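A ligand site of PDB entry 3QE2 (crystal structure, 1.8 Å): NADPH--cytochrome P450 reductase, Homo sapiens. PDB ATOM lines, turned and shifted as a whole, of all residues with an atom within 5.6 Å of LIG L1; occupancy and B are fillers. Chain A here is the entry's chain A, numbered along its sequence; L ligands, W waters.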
ATOM      1  N   TYR A 119      -0.546  27.146 -18.205  1.00  0.00           N
ATOM      2  CA  TYR A 119       0.738  26.541 -18.525  1.00  0.00           C
ATOM      3  C   TYR A 119       1.886  27.392 -17.977  1.00  0.00           C
ATOM      4  O   TYR A 119       1.720  28.571 -17.723  1.00  0.00           O
ATOM      5  CB  TYR A 119       0.869  26.387 -20.043  1.00  0.00           C
ATOM      6  CG  TYR A 119      -0.017  25.309 -20.612  1.00  0.00           C
ATOM      7  CD1 TYR A 119       0.363  23.970 -20.569  1.00  0.00           C
ATOM      8  CD2 TYR A 119      -1.253  25.626 -21.170  1.00  0.00           C
ATOM      9  CE1 TYR A 119      -0.470  22.963 -21.069  1.00  0.00           C
ATOM     10  CE2 TYR A 119      -2.095  24.637 -21.678  1.00  0.00           C
ATOM     11  CZ  TYR A 119      -1.693  23.313 -21.620  1.00  0.00           C
ATOM     12  OH  TYR A 119      -2.520  22.328 -22.112  1.00  0.00           O
ATOM     13  N   HIS A 260       2.054  10.884 -26.055  1.00  0.00           N
ATOM     14  CA  HIS A 260       0.618  11.015 -26.201  1.00  0.00           C
ATOM     15  C   HIS A 260       0.150  10.263 -27.434  1.00  0.00           C
ATOM     16  O   HIS A 260       0.884  10.159 -28.413  1.00  0.00           O
ATOM     17  CB  HIS A 260       0.234  12.488 -26.334  1.00  0.00           C
ATOM     18  CG  HIS A 260       0.644  13.324 -25.165  1.00  0.00           C
ATOM     19  ND1 HIS A 260       0.128  13.146 -23.903  1.00  0.00           N
ATOM     20  CD2 HIS A 260       1.540  14.341 -25.070  1.00  0.00           C
ATOM     21  CE1 HIS A 260       0.691  14.010 -23.073  1.00  0.00           C
ATOM     22  NE2 HIS A 260       1.543  14.743 -23.755  1.00  0.00           N
ATOM     23  N   THR A 319     -19.902  20.256 -32.258  1.00  0.00           N
ATOM     24  CA  THR A 319     -20.182  20.274 -30.834  1.00  0.00           C
ATOM     25  C   THR A 319     -19.650  21.468 -30.050  1.00  0.00           C
ATOM     26  O   THR A 319     -20.235  21.874 -29.058  1.00  0.00           O
ATOM     27  CB  THR A 319     -19.652  18.996 -30.187  1.00  0.00           C
ATOM     28  OG1 THR A 319     -18.303  18.776 -30.613  1.00  0.00           O
ATOM     29  CG2 THR A 319     -20.511  17.804 -30.600  1.00  0.00           C
ATOM     30  N   ASN A 320     -18.532  22.032 -30.493  1.00  0.00           N
ATOM     31  CA  ASN A 320     -17.967  23.182 -29.792  1.00  0.00           C
ATOM     32  C   ASN A 320     -18.807  24.436 -29.969  1.00  0.00           C
ATOM     33  O   ASN A 320     -19.340  24.694 -31.045  1.00  0.00           O
ATOM     34  CB  ASN A 320     -16.552  23.480 -30.289  1.00  0.00           C
ATOM     35  CG  ASN A 320     -15.503  23.044 -29.311  1.00  0.00           C
ATOM     36  OD1 ASN A 320     -15.011  21.915 -29.371  1.00  0.00           O
ATOM     37  ND2 ASN A 320     -15.144  23.945 -28.397  1.00  0.00           N
ATOM     38  N   ARG A 365     -23.085  26.529 -23.331  1.00  0.00           N
ATOM     39  CA  ARG A 365     -22.482  25.459 -24.124  1.00  0.00           C
ATOM     40  C   ARG A 365     -23.355  25.036 -25.310  1.00  0.00           C
ATOM     41  O   ARG A 365     -23.524  23.849 -25.598  1.00  0.00           O
ATOM     42  CB  ARG A 365     -22.215  24.227 -23.249  1.00  0.00           C
ATOM     43  CG  ARG A 365     -21.184  24.452 -22.146  1.00  0.00           C
ATOM     44  CD  ARG A 365     -19.785  24.615 -22.694  1.00  0.00           C
ATOM     45  NE  ARG A 365     -18.785  24.554 -21.630  1.00  0.00           N
ATOM     46  CZ  ARG A 365     -18.310  25.609 -20.967  1.00  0.00           C
ATOM     47  NH1 ARG A 365     -17.400  25.429 -20.004  1.00  0.00           N
ATOM     48  NH2 ARG A 365     -18.710  26.835 -21.268  1.00  0.00           N
ATOM     49  N   ARG A 395      -8.023  14.184 -30.601  1.00  0.00           N
ATOM     50  CA  ARG A 395      -7.980  14.384 -29.146  1.00  0.00           C
ATOM     51  C   ARG A 395      -6.736  13.641 -28.683  1.00  0.00           C
ATOM     52  O   ARG A 395      -6.410  12.580 -29.224  1.00  0.00           O
ATOM     53  CB  ARG A 395      -9.214  13.783 -28.470  1.00  0.00           C
ATOM     54  CG  ARG A 395     -10.351  14.764 -28.249  1.00  0.00           C
ATOM     55  CD  ARG A 395     -11.013  15.220 -29.553  1.00  0.00           C
ATOM     56  NE  ARG A 395     -12.185  16.023 -29.231  1.00  0.00           N
ATOM     57  CZ  ARG A 395     -12.760  16.900 -30.051  1.00  0.00           C
ATOM     58  NH1 ARG A 395     -13.821  17.579 -29.640  1.00  0.00           N
ATOM     59  NH2 ARG A 395     -12.267  17.088 -31.274  1.00  0.00           N
ATOM     60  N   TYR A 396      -6.059  14.173 -27.675  1.00  0.00           N
ATOM     61  CA  TYR A 396      -4.836  13.544 -27.162  1.00  0.00           C
ATOM     62  C   TYR A 396      -5.076  12.831 -25.829  1.00  0.00           C
ATOM     63  O   TYR A 396      -5.836  13.298 -24.992  1.00  0.00           O
ATOM     64  CB  TYR A 396      -3.763  14.598 -26.943  1.00  0.00           C
ATOM     65  CG  TYR A 396      -3.449  15.416 -28.170  1.00  0.00           C
ATOM     66  CD1 TYR A 396      -2.841  14.830 -29.278  1.00  0.00           C
ATOM     67  CD2 TYR A 396      -3.784  16.760 -28.238  1.00  0.00           C
ATOM     68  CE1 TYR A 396      -2.578  15.572 -30.429  1.00  0.00           C
ATOM     69  CE2 TYR A 396      -3.523  17.512 -29.387  1.00  0.00           C
ATOM     70  CZ  TYR A 396      -2.914  16.903 -30.475  1.00  0.00           C
ATOM     71  OH  TYR A 396      -2.667  17.630 -31.622  1.00  0.00           O
ATOM     72  N   TYR A 397      -4.406  11.696 -25.661  1.00  0.00           N
ATOM     73  CA  TYR A 397      -4.505  10.928 -24.424  1.00  0.00           C
ATOM     74  C   TYR A 397      -3.092  10.541 -24.005  1.00  0.00           C
ATOM     75  O   TYR A 397      -2.236  10.248 -24.847  1.00  0.00           O
ATOM     76  CB  TYR A 397      -5.376   9.691 -24.636  1.00  0.00           C
ATOM     77  CG  TYR A 397      -6.812  10.073 -24.881  1.00  0.00           C
ATOM     78  CD1 TYR A 397      -7.654  10.398 -23.812  1.00  0.00           C
ATOM     79  CD2 TYR A 397      -7.274  10.290 -26.168  1.00  0.00           C
ATOM     80  CE1 TYR A 397      -8.914  10.933 -24.034  1.00  0.00           C
ATOM     81  CE2 TYR A 397      -8.527  10.828 -26.402  1.00  0.00           C
ATOM     82  CZ  TYR A 397      -9.345  11.149 -25.330  1.00  0.00           C
ATOM     83  OH  TYR A 397     -10.550  11.765 -25.577  1.00  0.00           O
ATOM     84  N   SER A 398      -2.831  10.558 -22.705  1.00  0.00           N
ATOM     85  CA  SER A 398      -1.517  10.199 -22.224  1.00  0.00           C
ATOM     86  C   SER A 398      -1.410   8.683 -22.227  1.00  0.00           C
ATOM     87  O   SER A 398      -2.167   8.007 -21.530  1.00  0.00           O
ATOM     88  CB  SER A 398      -1.320  10.761 -20.818  1.00  0.00           C
ATOM     89  OG  SER A 398      -1.560  12.155 -20.808  1.00  0.00           O
ATOM     90  N   CYS A 413      -6.351   5.721 -20.726  1.00  0.00           N
ATOM     91  CA  CYS A 413      -7.157   5.821 -19.516  1.00  0.00           C
ATOM     92  C   CYS A 413      -7.935   7.124 -19.690  1.00  0.00           C
ATOM     93  O   CYS A 413      -7.350   8.209 -19.687  1.00  0.00           O
ATOM     94  CB  CYS A 413      -6.291   5.920 -18.262  1.00  0.00           C
ATOM     95  SG  CYS A 413      -7.270   6.340 -16.783  1.00  0.00           S
ATOM     96  N   ALA A 414      -9.258   7.027 -19.844  1.00  0.00           N
ATOM     97  CA  ALA A 414     -10.055   8.227 -20.077  1.00  0.00           C
ATOM     98  C   ALA A 414     -11.388   8.281 -19.335  1.00  0.00           C
ATOM     99  O   ALA A 414     -11.981   7.253 -19.010  1.00  0.00           O
ATOM    100  CB  ALA A 414     -10.324   8.365 -21.570  1.00  0.00           C
ATOM    101  N   VAL A 415     -11.848   9.502 -19.074  1.00  0.00           N
ATOM    102  CA  VAL A 415     -13.134   9.704 -18.417  1.00  0.00           C
ATOM    103  C   VAL A 415     -14.104  10.242 -19.459  1.00  0.00           C
ATOM    104  O   VAL A 415     -13.779  11.177 -20.196  1.00  0.00           O
ATOM    105  CB  VAL A 415     -13.032  10.689 -17.214  1.00  0.00           C
ATOM    106  CG1 VAL A 415     -12.391  11.983 -17.642  1.00  0.00           C
ATOM    107  CG2 VAL A 415     -14.421  10.943 -16.629  1.00  0.00           C
ATOM    108  N   VAL A 417     -16.999  12.306 -21.105  1.00  0.00           N
ATOM    109  CA  VAL A 417     -17.583  13.611 -20.877  1.00  0.00           C
ATOM    110  C   VAL A 417     -19.086  13.585 -21.194  1.00  0.00           C
ATOM    111  O   VAL A 417     -19.487  13.226 -22.303  1.00  0.00           O
ATOM    112  CB  VAL A 417     -16.865  14.692 -21.752  1.00  0.00           C
ATOM    113  CG1 VAL A 417     -17.645  16.006 -21.736  1.00  0.00           C
ATOM    114  CG2 VAL A 417     -15.460  14.928 -21.212  1.00  0.00           C
ATOM    115  N   TYR A 419     -22.620  15.921 -19.681  1.00  0.00           N
ATOM    116  CA  TYR A 419     -23.159  16.831 -18.692  1.00  0.00           C
ATOM    117  C   TYR A 419     -24.403  17.555 -19.175  1.00  0.00           C
ATOM    118  O   TYR A 419     -24.698  17.570 -20.371  1.00  0.00           O
ATOM    119  CB  TYR A 419     -22.102  17.874 -18.321  1.00  0.00           C
ATOM    120  CG  TYR A 419     -21.593  18.660 -19.515  1.00  0.00           C
ATOM    121  CD1 TYR A 419     -20.664  18.099 -20.395  1.00  0.00           C
ATOM    122  CD2 TYR A 419     -22.076  19.941 -19.779  1.00  0.00           C
ATOM    123  CE1 TYR A 419     -20.225  18.803 -21.506  1.00  0.00           C
ATOM    124  CE2 TYR A 419     -21.640  20.646 -20.900  1.00  0.00           C
ATOM    125  CZ  TYR A 419     -20.724  20.079 -21.755  1.00  0.00           C
ATOM    126  OH  TYR A 419     -20.291  20.771 -22.865  1.00  0.00           O
ATOM    127  N   LYS A 428     -22.455  15.627 -24.934  1.00  0.00           N
ATOM    128  CA  LYS A 428     -21.617  14.452 -24.828  1.00  0.00           C
ATOM    129  C   LYS A 428     -20.295  14.715 -25.527  1.00  0.00           C
ATOM    130  O   LYS A 428     -20.274  15.149 -26.684  1.00  0.00           O
ATOM    131  CB  LYS A 428     -22.311  13.249 -25.469  1.00  0.00           C
ATOM    132  CG  LYS A 428     -23.555  12.788 -24.755  1.00  0.00           C
ATOM    133  CD  LYS A 428     -24.094  11.522 -25.382  1.00  0.00           C
ATOM    134  CE  LYS A 428     -25.334  11.019 -24.661  1.00  0.00           C
ATOM    135  NZ  LYS A 428     -25.881   9.799 -25.337  1.00  0.00           N
ATOM    136  N   GLY A 429     -19.188  14.452 -24.835  1.00  0.00           N
ATOM    137  CA  GLY A 429     -17.866  14.658 -25.410  1.00  0.00           C
ATOM    138  C   GLY A 429     -17.698  13.794 -26.641  1.00  0.00           C
ATOM    139  O   GLY A 429     -18.006  12.608 -26.626  1.00  0.00           O
ATOM    140  N   VAL A 430     -17.181  14.391 -27.715  1.00  0.00           N
ATOM    141  CA  VAL A 430     -17.002  13.679 -28.967  1.00  0.00           C
ATOM    142  C   VAL A 430     -16.120  12.428 -28.907  1.00  0.00           C
ATOM    143  O   VAL A 430     -16.594  11.330 -29.174  1.00  0.00           O
ATOM    144  CB  VAL A 430     -16.446  14.614 -30.067  1.00  0.00           C
ATOM    145  CG1 VAL A 430     -16.379  13.868 -31.400  1.00  0.00           C
ATOM    146  CG2 VAL A 430     -17.330  15.859 -30.178  1.00  0.00           C
ATOM    147  N   ALA A 431     -14.848  12.594 -28.559  1.00  0.00           N
ATOM    148  CA  ALA A 431     -13.948  11.456 -28.534  1.00  0.00           C
ATOM    149  C   ALA A 431     -14.248  10.390 -27.483  1.00  0.00           C
ATOM    150  O   ALA A 431     -14.185   9.196 -27.769  1.00  0.00           O
ATOM    151  CB  ALA A 431     -12.495  11.926 -28.391  1.00  0.00           C
ATOM    152  N   THR A 432     -14.584  10.811 -26.263  1.00  0.00           N
ATOM    153  CA  THR A 432     -14.838   9.842 -25.214  1.00  0.00           C
ATOM    154  C   THR A 432     -16.077   8.989 -25.410  1.00  0.00           C
ATOM    155  O   THR A 432     -16.060   7.792 -25.118  1.00  0.00           O
ATOM    156  CB  THR A 432     -14.843  10.515 -23.818  1.00  0.00           C
ATOM    157  OG1 THR A 432     -15.794  11.590 -23.787  1.00  0.00           O
ATOM    158  CG2 THR A 432     -13.458  11.073 -23.516  1.00  0.00           C
ATOM    159  N   ASN A 433     -17.154   9.566 -25.927  1.00  0.00           N
ATOM    160  CA  ASN A 433     -18.353   8.738 -26.145  1.00  0.00           C
ATOM    161  C   ASN A 433     -18.160   7.816 -27.353  1.00  0.00           C
ATOM    162  O   ASN A 433     -18.700   6.704 -27.381  1.00  0.00           O
ATOM    163  CB  ASN A 433     -19.570   9.644 -26.309  1.00  0.00           C
ATOM    164  CG  ASN A 433     -20.096  10.123 -24.967  1.00  0.00           C
ATOM    165  OD1 ASN A 433     -20.901   9.449 -24.319  1.00  0.00           O
ATOM    166  ND2 ASN A 433     -19.610  11.279 -24.525  1.00  0.00           N
ATOM    167  N   THR A 476      -7.759  10.903 -13.879  1.00  0.00           N
ATOM    168  CA  THR A 476      -7.159  10.347 -15.088  1.00  0.00           C
ATOM    169  C   THR A 476      -5.709  10.795 -15.237  1.00  0.00           C
ATOM    170  O   THR A 476      -4.987  10.355 -16.135  1.00  0.00           O
ATOM    171  CB  THR A 476      -7.962  10.755 -16.330  1.00  0.00           C
ATOM    172  OG1 THR A 476      -8.187  12.174 -16.314  1.00  0.00           O
ATOM    173  CG2 THR A 476      -9.286  10.018 -16.361  1.00  0.00           C
ATOM    174  N   ALA A 479      -2.859   8.278 -15.616  1.00  0.00           N
ATOM    175  CA  ALA A 479      -2.556   7.635 -16.893  1.00  0.00           C
ATOM    176  C   ALA A 479      -1.104   7.300 -17.238  1.00  0.00           C
ATOM    177  O   ALA A 479      -0.737   6.128 -17.323  1.00  0.00           O
ATOM    178  CB  ALA A 479      -3.196   8.454 -18.029  1.00  0.00           C
ATOM    179  N   ASP A 615       2.443  17.219 -17.440  1.00  0.00           N
ATOM    180  CA  ASP A 615       1.588  16.684 -18.499  1.00  0.00           C
ATOM    181  C   ASP A 615       0.189  17.051 -18.013  1.00  0.00           C
ATOM    182  O   ASP A 615      -0.562  16.190 -17.531  1.00  0.00           O
ATOM    183  CB  ASP A 615       1.714  15.166 -18.623  1.00  0.00           C
ATOM    184  CG  ASP A 615       0.826  14.595 -19.724  1.00  0.00           C
ATOM    185  OD1 ASP A 615       0.686  13.350 -19.793  1.00  0.00           O
ATOM    186  OD2 ASP A 615       0.287  15.375 -20.526  1.00  0.00           O
ATOM    187  N   VAL A 616      -0.148  18.322 -18.091  1.00  0.00           N
ATOM    188  CA  VAL A 616      -1.441  18.783 -17.625  1.00  0.00           C
ATOM    189  C   VAL A 616      -2.320  19.313 -18.736  1.00  0.00           C
ATOM    190  O   VAL A 616      -1.830  19.743 -19.785  1.00  0.00           O
ATOM    191  CB  VAL A 616      -1.274  19.872 -16.533  1.00  0.00           C
ATOM    192  CG1 VAL A 616      -0.592  19.256 -15.332  1.00  0.00           C
ATOM    193  CG2 VAL A 616      -0.461  21.048 -17.058  1.00  0.00           C
ATOM    194  N   TRP A 617      -3.630  19.261 -18.506  1.00  0.00           N
ATOM    195  CA  TRP A 617      -4.601  19.710 -19.497  1.00  0.00           C
ATOM    196  C   TRP A 617      -5.892  20.172 -18.843  1.00  0.00           C
ATOM    197  O   TRP A 617      -6.089  19.987 -17.648  1.00  0.00           O
ATOM    198  CB  TRP A 617      -4.909  18.567 -20.464  1.00  0.00           C
ATOM    199  CG  TRP A 617      -5.573  17.379 -19.817  1.00  0.00           C
ATOM    200  CD1 TRP A 617      -6.915  17.196 -19.612  1.00  0.00           C
ATOM    201  CD2 TRP A 617      -4.930  16.209 -19.296  1.00  0.00           C
ATOM    202  NE1 TRP A 617      -7.148  15.988 -19.003  1.00  0.00           N
ATOM    203  CE2 TRP A 617      -5.941  15.357 -18.798  1.00  0.00           C
ATOM    204  CE3 TRP A 617      -3.596  15.794 -19.210  1.00  0.00           C
ATOM    205  CZ2 TRP A 617      -5.659  14.119 -18.211  1.00  0.00           C
ATOM    206  CZ3 TRP A 617      -3.308  14.560 -18.634  1.00  0.00           C
ATOM    207  CH2 TRP A 617      -4.339  13.733 -18.140  1.00  0.00           C
ATOM    208  N   SER A 618      -6.760  20.777 -19.653  1.00  0.00           N
ATOM    209  CA  SER A 618      -8.055  21.257 -19.175  1.00  0.00           C
ATOM    210  C   SER A 618      -9.167  20.534 -19.940  1.00  0.00           C
ATOM    211  O   SER A 618      -8.873  19.948 -21.004  1.00  0.00           O
ATOM    212  CB  SER A 618      -8.187  22.761 -19.416  1.00  0.00           C
ATOM    213  OG  SER A 618      -7.236  23.479 -18.644  1.00  0.00           O
ATOM    214  OXT SER A 618     -10.326  20.572 -19.472  1.00  0.00           O
HETATM  215  P1  LIG L   1     -15.201  17.383 -26.130  1.00  0.00           P
HETATM  216  O1  LIG L   1     -16.359  17.112 -27.048  1.00  0.00           O
HETATM  217  O2  LIG L   1     -14.012  18.006 -26.750  1.00  0.00           O
HETATM  218  O3  LIG L   1     -15.716  18.292 -25.064  1.00  0.00           O
HETATM  219  C1  LIG L   1     -14.886  18.818 -23.988  1.00  0.00           C
HETATM  220  C2  LIG L   1     -15.359  20.176 -23.480  1.00  0.00           C
HETATM  221  O4  LIG L   1     -16.642  20.005 -22.842  1.00  0.00           O
HETATM  222  C3  LIG L   1     -14.508  20.808 -22.365  1.00  0.00           C
HETATM  223  O5  LIG L   1     -13.417  21.541 -22.901  1.00  0.00           O
HETATM  224  C4  LIG L   1     -15.480  21.814 -21.744  1.00  0.00           C
HETATM  225  O6  LIG L   1     -15.645  23.096 -22.440  1.00  0.00           O
HETATM  226  C5  LIG L   1     -16.783  20.990 -21.795  1.00  0.00           C
HETATM  227  N1  LIG L   1     -17.189  20.340 -20.515  1.00  0.00           N
HETATM  228  C6  LIG L   1     -16.879  19.120 -19.925  1.00  0.00           C
HETATM  229  N2  LIG L   1     -17.509  18.905 -18.713  1.00  0.00           N
HETATM  230  C7  LIG L   1     -18.251  20.044 -18.536  1.00  0.00           C
HETATM  231  C8  LIG L   1     -19.157  20.533 -17.507  1.00  0.00           C
HETATM  232  N3  LIG L   1     -19.455  19.805 -16.387  1.00  0.00           N
HETATM  233  N4  LIG L   1     -19.710  21.791 -17.740  1.00  0.00           N
HETATM  234  C9  LIG L   1     -19.500  22.613 -18.800  1.00  0.00           C
HETATM  235  N5  LIG L   1     -18.671  22.260 -19.833  1.00  0.00           N
HETATM  236  C10 LIG L   1     -18.064  20.959 -19.649  1.00  0.00           C
HETATM  237  N6  LIG L   1      -8.272  12.936 -21.070  1.00  0.00           N
HETATM  238  C11 LIG L   1      -8.358  11.726 -20.443  1.00  0.00           C
HETATM  239  O7  LIG L   1      -9.454  11.334 -20.076  1.00  0.00           O
HETATM  240  N7  LIG L   1      -7.206  11.031 -20.276  1.00  0.00           N
HETATM  241  C12 LIG L   1      -5.892  11.404 -20.667  1.00  0.00           C
HETATM  242  O8  LIG L   1      -4.938  10.658 -20.451  1.00  0.00           O
HETATM  243  C13 LIG L   1      -5.809  12.709 -21.312  1.00  0.00           C
HETATM  244  N8  LIG L   1      -4.530  13.124 -21.702  1.00  0.00           N
HETATM  245  C14 LIG L   1      -4.476  14.376 -22.319  1.00  0.00           C
HETATM  246  C15 LIG L   1      -3.156  14.857 -22.720  1.00  0.00           C
HETATM  247  C16 LIG L   1      -2.978  16.115 -23.353  1.00  0.00           C
HETATM  248  C17 LIG L   1      -1.570  16.589 -23.760  1.00  0.00           C
HETATM  249  C18 LIG L   1      -4.185  16.939 -23.605  1.00  0.00           C
HETATM  250  C19 LIG L   1      -4.132  18.312 -24.281  1.00  0.00           C
HETATM  251  C20 LIG L   1      -5.455  16.508 -23.239  1.00  0.00           C
HETATM  252  C21 LIG L   1      -5.658  15.241 -22.588  1.00  0.00           C
HETATM  253  N9  LIG L   1      -6.971  14.707 -22.148  1.00  0.00           N
HETATM  254  C22 LIG L   1      -7.049  13.455 -21.504  1.00  0.00           C
HETATM  255  C23 LIG L   1      -8.270  15.416 -22.354  1.00  0.00           C
HETATM  256  C24 LIG L   1      -8.585  14.742 -23.799  1.00  0.00           C
HETATM  257  O9  LIG L   1      -7.666  15.092 -24.918  1.00  0.00           O
HETATM  258  C25 LIG L   1     -10.028  15.301 -24.247  1.00  0.00           C
HETATM  259  O10 LIG L   1     -10.098  16.758 -24.183  1.00  0.00           O
HETATM  260  C26 LIG L   1     -11.203  14.782 -23.399  1.00  0.00           C
HETATM  261  O11 LIG L   1     -11.145  13.341 -23.449  1.00  0.00           O
HETATM  262  C27 LIG L   1     -12.496  15.238 -23.853  1.00  0.00           C
HETATM  263  O12 LIG L   1     -12.752  15.077 -25.253  1.00  0.00           O
HETATM  264  P2  LIG L   1     -14.117  14.869 -25.846  1.00  0.00           P
HETATM  265  O13 LIG L   1     -14.808  13.645 -25.328  1.00  0.00           O
HETATM  266  O14 LIG L   1     -13.874  14.816 -27.322  1.00  0.00           O
HETATM  267  O15 LIG L   1     -14.806  16.183 -25.304  1.00  0.00           O
HETATM  268  N1  LG2 L   2      -0.231  27.674 -24.102  1.00  0.00           N
HETATM  269  C1  LG2 L   2       0.752  28.413 -23.528  1.00  0.00           C
HETATM  270  O1  LG2 L   2       0.588  29.613 -23.357  1.00  0.00           O
HETATM  271  N2  LG2 L   2       1.917  27.795 -23.164  1.00  0.00           N
HETATM  272  C2  LG2 L   2       2.184  26.424 -23.317  1.00  0.00           C
HETATM  273  O2  LG2 L   2       3.294  26.079 -22.920  1.00  0.00           O
HETATM  274  C3  LG2 L   2       1.140  25.608 -23.916  1.00  0.00           C
HETATM  275  N3  LG2 L   2       1.377  24.229 -24.071  1.00  0.00           N
HETATM  276  C4  LG2 L   2       0.343  23.517 -24.640  1.00  0.00           C
HETATM  277  C5  LG2 L   2       0.581  22.096 -24.796  1.00  0.00           C
HETATM  278  C6  LG2 L   2      -0.380  21.236 -25.348  1.00  0.00           C
HETATM  279  C7  LG2 L   2       0.009  19.746 -25.437  1.00  0.00           C
HETATM  280  C8  LG2 L   2      -1.697  21.769 -25.803  1.00  0.00           C
HETATM  281  C9  LG2 L   2      -2.823  20.912 -26.431  1.00  0.00           C
HETATM  282  C10 LG2 L   2      -1.943  23.126 -25.667  1.00  0.00           C
HETATM  283  C11 LG2 L   2      -0.953  24.055 -25.091  1.00  0.00           C
HETATM  284  N4  LG2 L   2      -1.139  25.518 -24.898  1.00  0.00           N
HETATM  285  C12 LG2 L   2      -0.057  26.323 -24.289  1.00  0.00           C
HETATM  286  C13 LG2 L   2      -2.370  26.123 -25.315  1.00  0.00           C
HETATM  287  C14 LG2 L   2      -2.458  26.451 -26.839  1.00  0.00           C
HETATM  288  O3  LG2 L   2      -1.343  27.280 -27.233  1.00  0.00           O
HETATM  289  C15 LG2 L   2      -3.813  27.063 -27.155  1.00  0.00           C
HETATM  290  O4  LG2 L   2      -4.795  26.032 -26.858  1.00  0.00           O
HETATM  291  C16 LG2 L   2      -3.884  27.447 -28.672  1.00  0.00           C
HETATM  292  O5  LG2 L   2      -5.227  28.035 -28.826  1.00  0.00           O
HETATM  293  C17 LG2 L   2      -3.795  26.279 -29.614  1.00  0.00           C
HETATM  294  O6  LG2 L   2      -3.796  26.723 -31.015  1.00  0.00           O
HETATM  295  P1  LG2 L   2      -3.948  25.777 -32.234  1.00  0.00           P
HETATM  296  O7  LG2 L   2      -5.347  25.220 -32.291  1.00  0.00           O
HETATM  297  O8  LG2 L   2      -2.867  24.771 -32.271  1.00  0.00           O
HETATM  298  O9  LG2 L   2      -3.811  26.723 -33.373  1.00  0.00           O
HETATM  299  O   HOH W   1     -10.965  18.397 -22.096  1.00  0.00           O
HETATM  300  O   HOH W   2     -14.095  25.048 -21.645  1.00  0.00           O
HETATM  301  O   HOH W   3     -11.296  18.128 -26.172  1.00  0.00           O
HETATM  302  O   HOH W   4     -17.220  24.155 -24.562  1.00  0.00           O
HETATM  303  O   HOH W   5      -4.783   7.939 -21.384  1.00  0.00           O
HETATM  304  O   HOH W   6     -16.831  19.402 -28.590  1.00  0.00           O
HETATM  305  O   HOH W   7     -11.211  20.457 -24.589  1.00  0.00           O
HETATM  306  O   HOH W   8     -12.644  23.348 -24.727  1.00  0.00           O
HETATM  307  O   HOH W   9     -13.797  20.844 -26.826  1.00  0.00           O
HETATM  308  O   HOH W  10      -7.002  16.950 -26.836  1.00  0.00           O
HETATM  309  O   HOH W  11      -7.962  18.696 -24.143  1.00  0.00           O
HETATM  310  O   HOH W  12     -19.124  17.896 -26.755  1.00  0.00           O
HETATM  311  O   HOH W  13      -9.320  14.232 -18.307  1.00  0.00           O
HETATM  312  O   HOH W  14     -18.764  19.598 -24.547  1.00  0.00           O
HETATM  313  O   HOH W  15     -22.891  22.129 -16.827  1.00  0.00           O
HETATM  314  O   HOH W  16     -11.581  12.720 -20.883  1.00  0.00           O
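The backbone NH (N) of Tyr 396 sits at hydrogen-bond distance from an oxygen (O9) of LIG L1 (3.3 Å). O of Tyr 396 lies within hydrogen-bond range of O9 of LIG L1 (2.6 Å). The side-chain hydroxyl (OH) of Tyr 397 lies within hydrogen-bond range of an oxygen (O11) of LIG L1 (2.7 Å). The backbone NH (N) of Ala 431 lies within hydrogen-bond range of an oxygen (O14) of LIG L1 (2.7 Å). The backbone NH (N) of Thr 432 lies within hydrogen-bond range of an oxygen (O13) of LIG L1 (3.0 Å). The side-chain hydroxyl (OG1) of Thr 432 lies within hydrogen-bond range of an oxygen (O13) of LIG L1 (2.8 Å). The guanidinium group (NE) of Arg 395 is in salt-bridge range of an oxygen (O14) of LIG L1, 2.8 Å away. O of Cys 413 is in hydrogen-bond range of N7 of LIG L1, 2.9 Å away. N5 of LIG L1 is in hydrogen-bond range of NE of Arg 365. An oxygen (O1) of LIG L1 lies within hydrogen-bond range of the backbone NH (N) of Val 430 (2.9 Å). O8 of LIG L1 sits at hydrogen-bond distance from N of Ser 398, at 3.1 Å. OG of Ser 398 is in hydrogen-bond range of N8 of LIG L1 (3.2 Å). N of Val 415 sits at hydrogen-bond distance from O7 of LIG L1 (3.2 Å).
OG1 of Thr 432 is in hydrogen-bond range of N of Val 417 (3.0 Å). OG of Ser 398 sits at hydrogen-bond distance from OD1 of Asp 615 (2.7 Å). N of Gly 429 is in hydrogen-bond range of O of Val 417. O of Gly 429 sits at hydrogen-bond distance from ND2 of Asn 433 (3.0 Å). The backbone carbonyl oxygen (O) of Val 417 is in hydrogen-bond range of the side-chain amide nitrogen (ND2) of Asn 433, 3.0 Å away.
N9 of LIG L1 sits close to NE1 of Trp 617, at 3.4 Å. His 260 touches LIG L1 (CE1 to C17, 3.5 Å). CA of Ala 414 touches O7 of LIG L1, 3.2 Å away. Val 417 touches LIG L1. CZ of Tyr 419 touches C10 of LIG L1, at 3.5 Å. Gly 429 touches LIG L1. Thr 476 touches LIG L1 (CG2 to O7, 3.9 Å). Ala 479 touches LIG L1 (CB to O8, 3.7 Å). OD2 of Asp 615 touches C17 of LIG L1, 3.9 Å away. Hydrophobic or aromatic side chains that line LIG L1: His 260, Tyr 396, Tyr 397, Ala 414, Val 415, Val 417, Tyr 419, Val 430, Ala 431, Ala 479 and Trp 617. Within 4 Å of LIG L1: His 260, Arg 365, Arg 395, Tyr 396, Tyr 397, Ser 398, Cys 413, Ala 414, Val 415, Val 417, Tyr 419, Gly 429, Val 430, Ala 431, Thr 432, Thr 476, Ala 479, Asp 615 and Trp 617. Along chain A the residues within 4 Å of LIG L1 span positions 260 to 617.
Water W16 lies within hydrogen-bond range of an oxygen (O7) of LIG L1 and the backbone carbonyl oxygen of Val 415. Water W14 bridges the side-chain hydroxyl (OH) of Tyr 419 and an oxygen (O4) of LIG L1. Water W6 lies within hydrogen-bond range of OG1 of Thr 319 (2.6 Å), O1 of LIG L1 (2.8 Å) and OD1 of Asn 320 (3.2 Å). Water W9 lies within hydrogen-bond range of an oxygen (O2) of LIG L1 (2.8 Å) and the side-chain amide oxygen of Asn 320 (3.0 Å). Water W5 lies within hydrogen-bond range of O of Ser 398 (2.6 Å), N of Cys 413 (2.8 Å) and O8 of LIG L1 (2.9 Å). Water W13 lies within hydrogen-bond range of NE1 of Trp 617 (2.9 Å), OG1 of Thr 476 (3.1 Å) and N6 of LIG L1 (3.2 Å).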
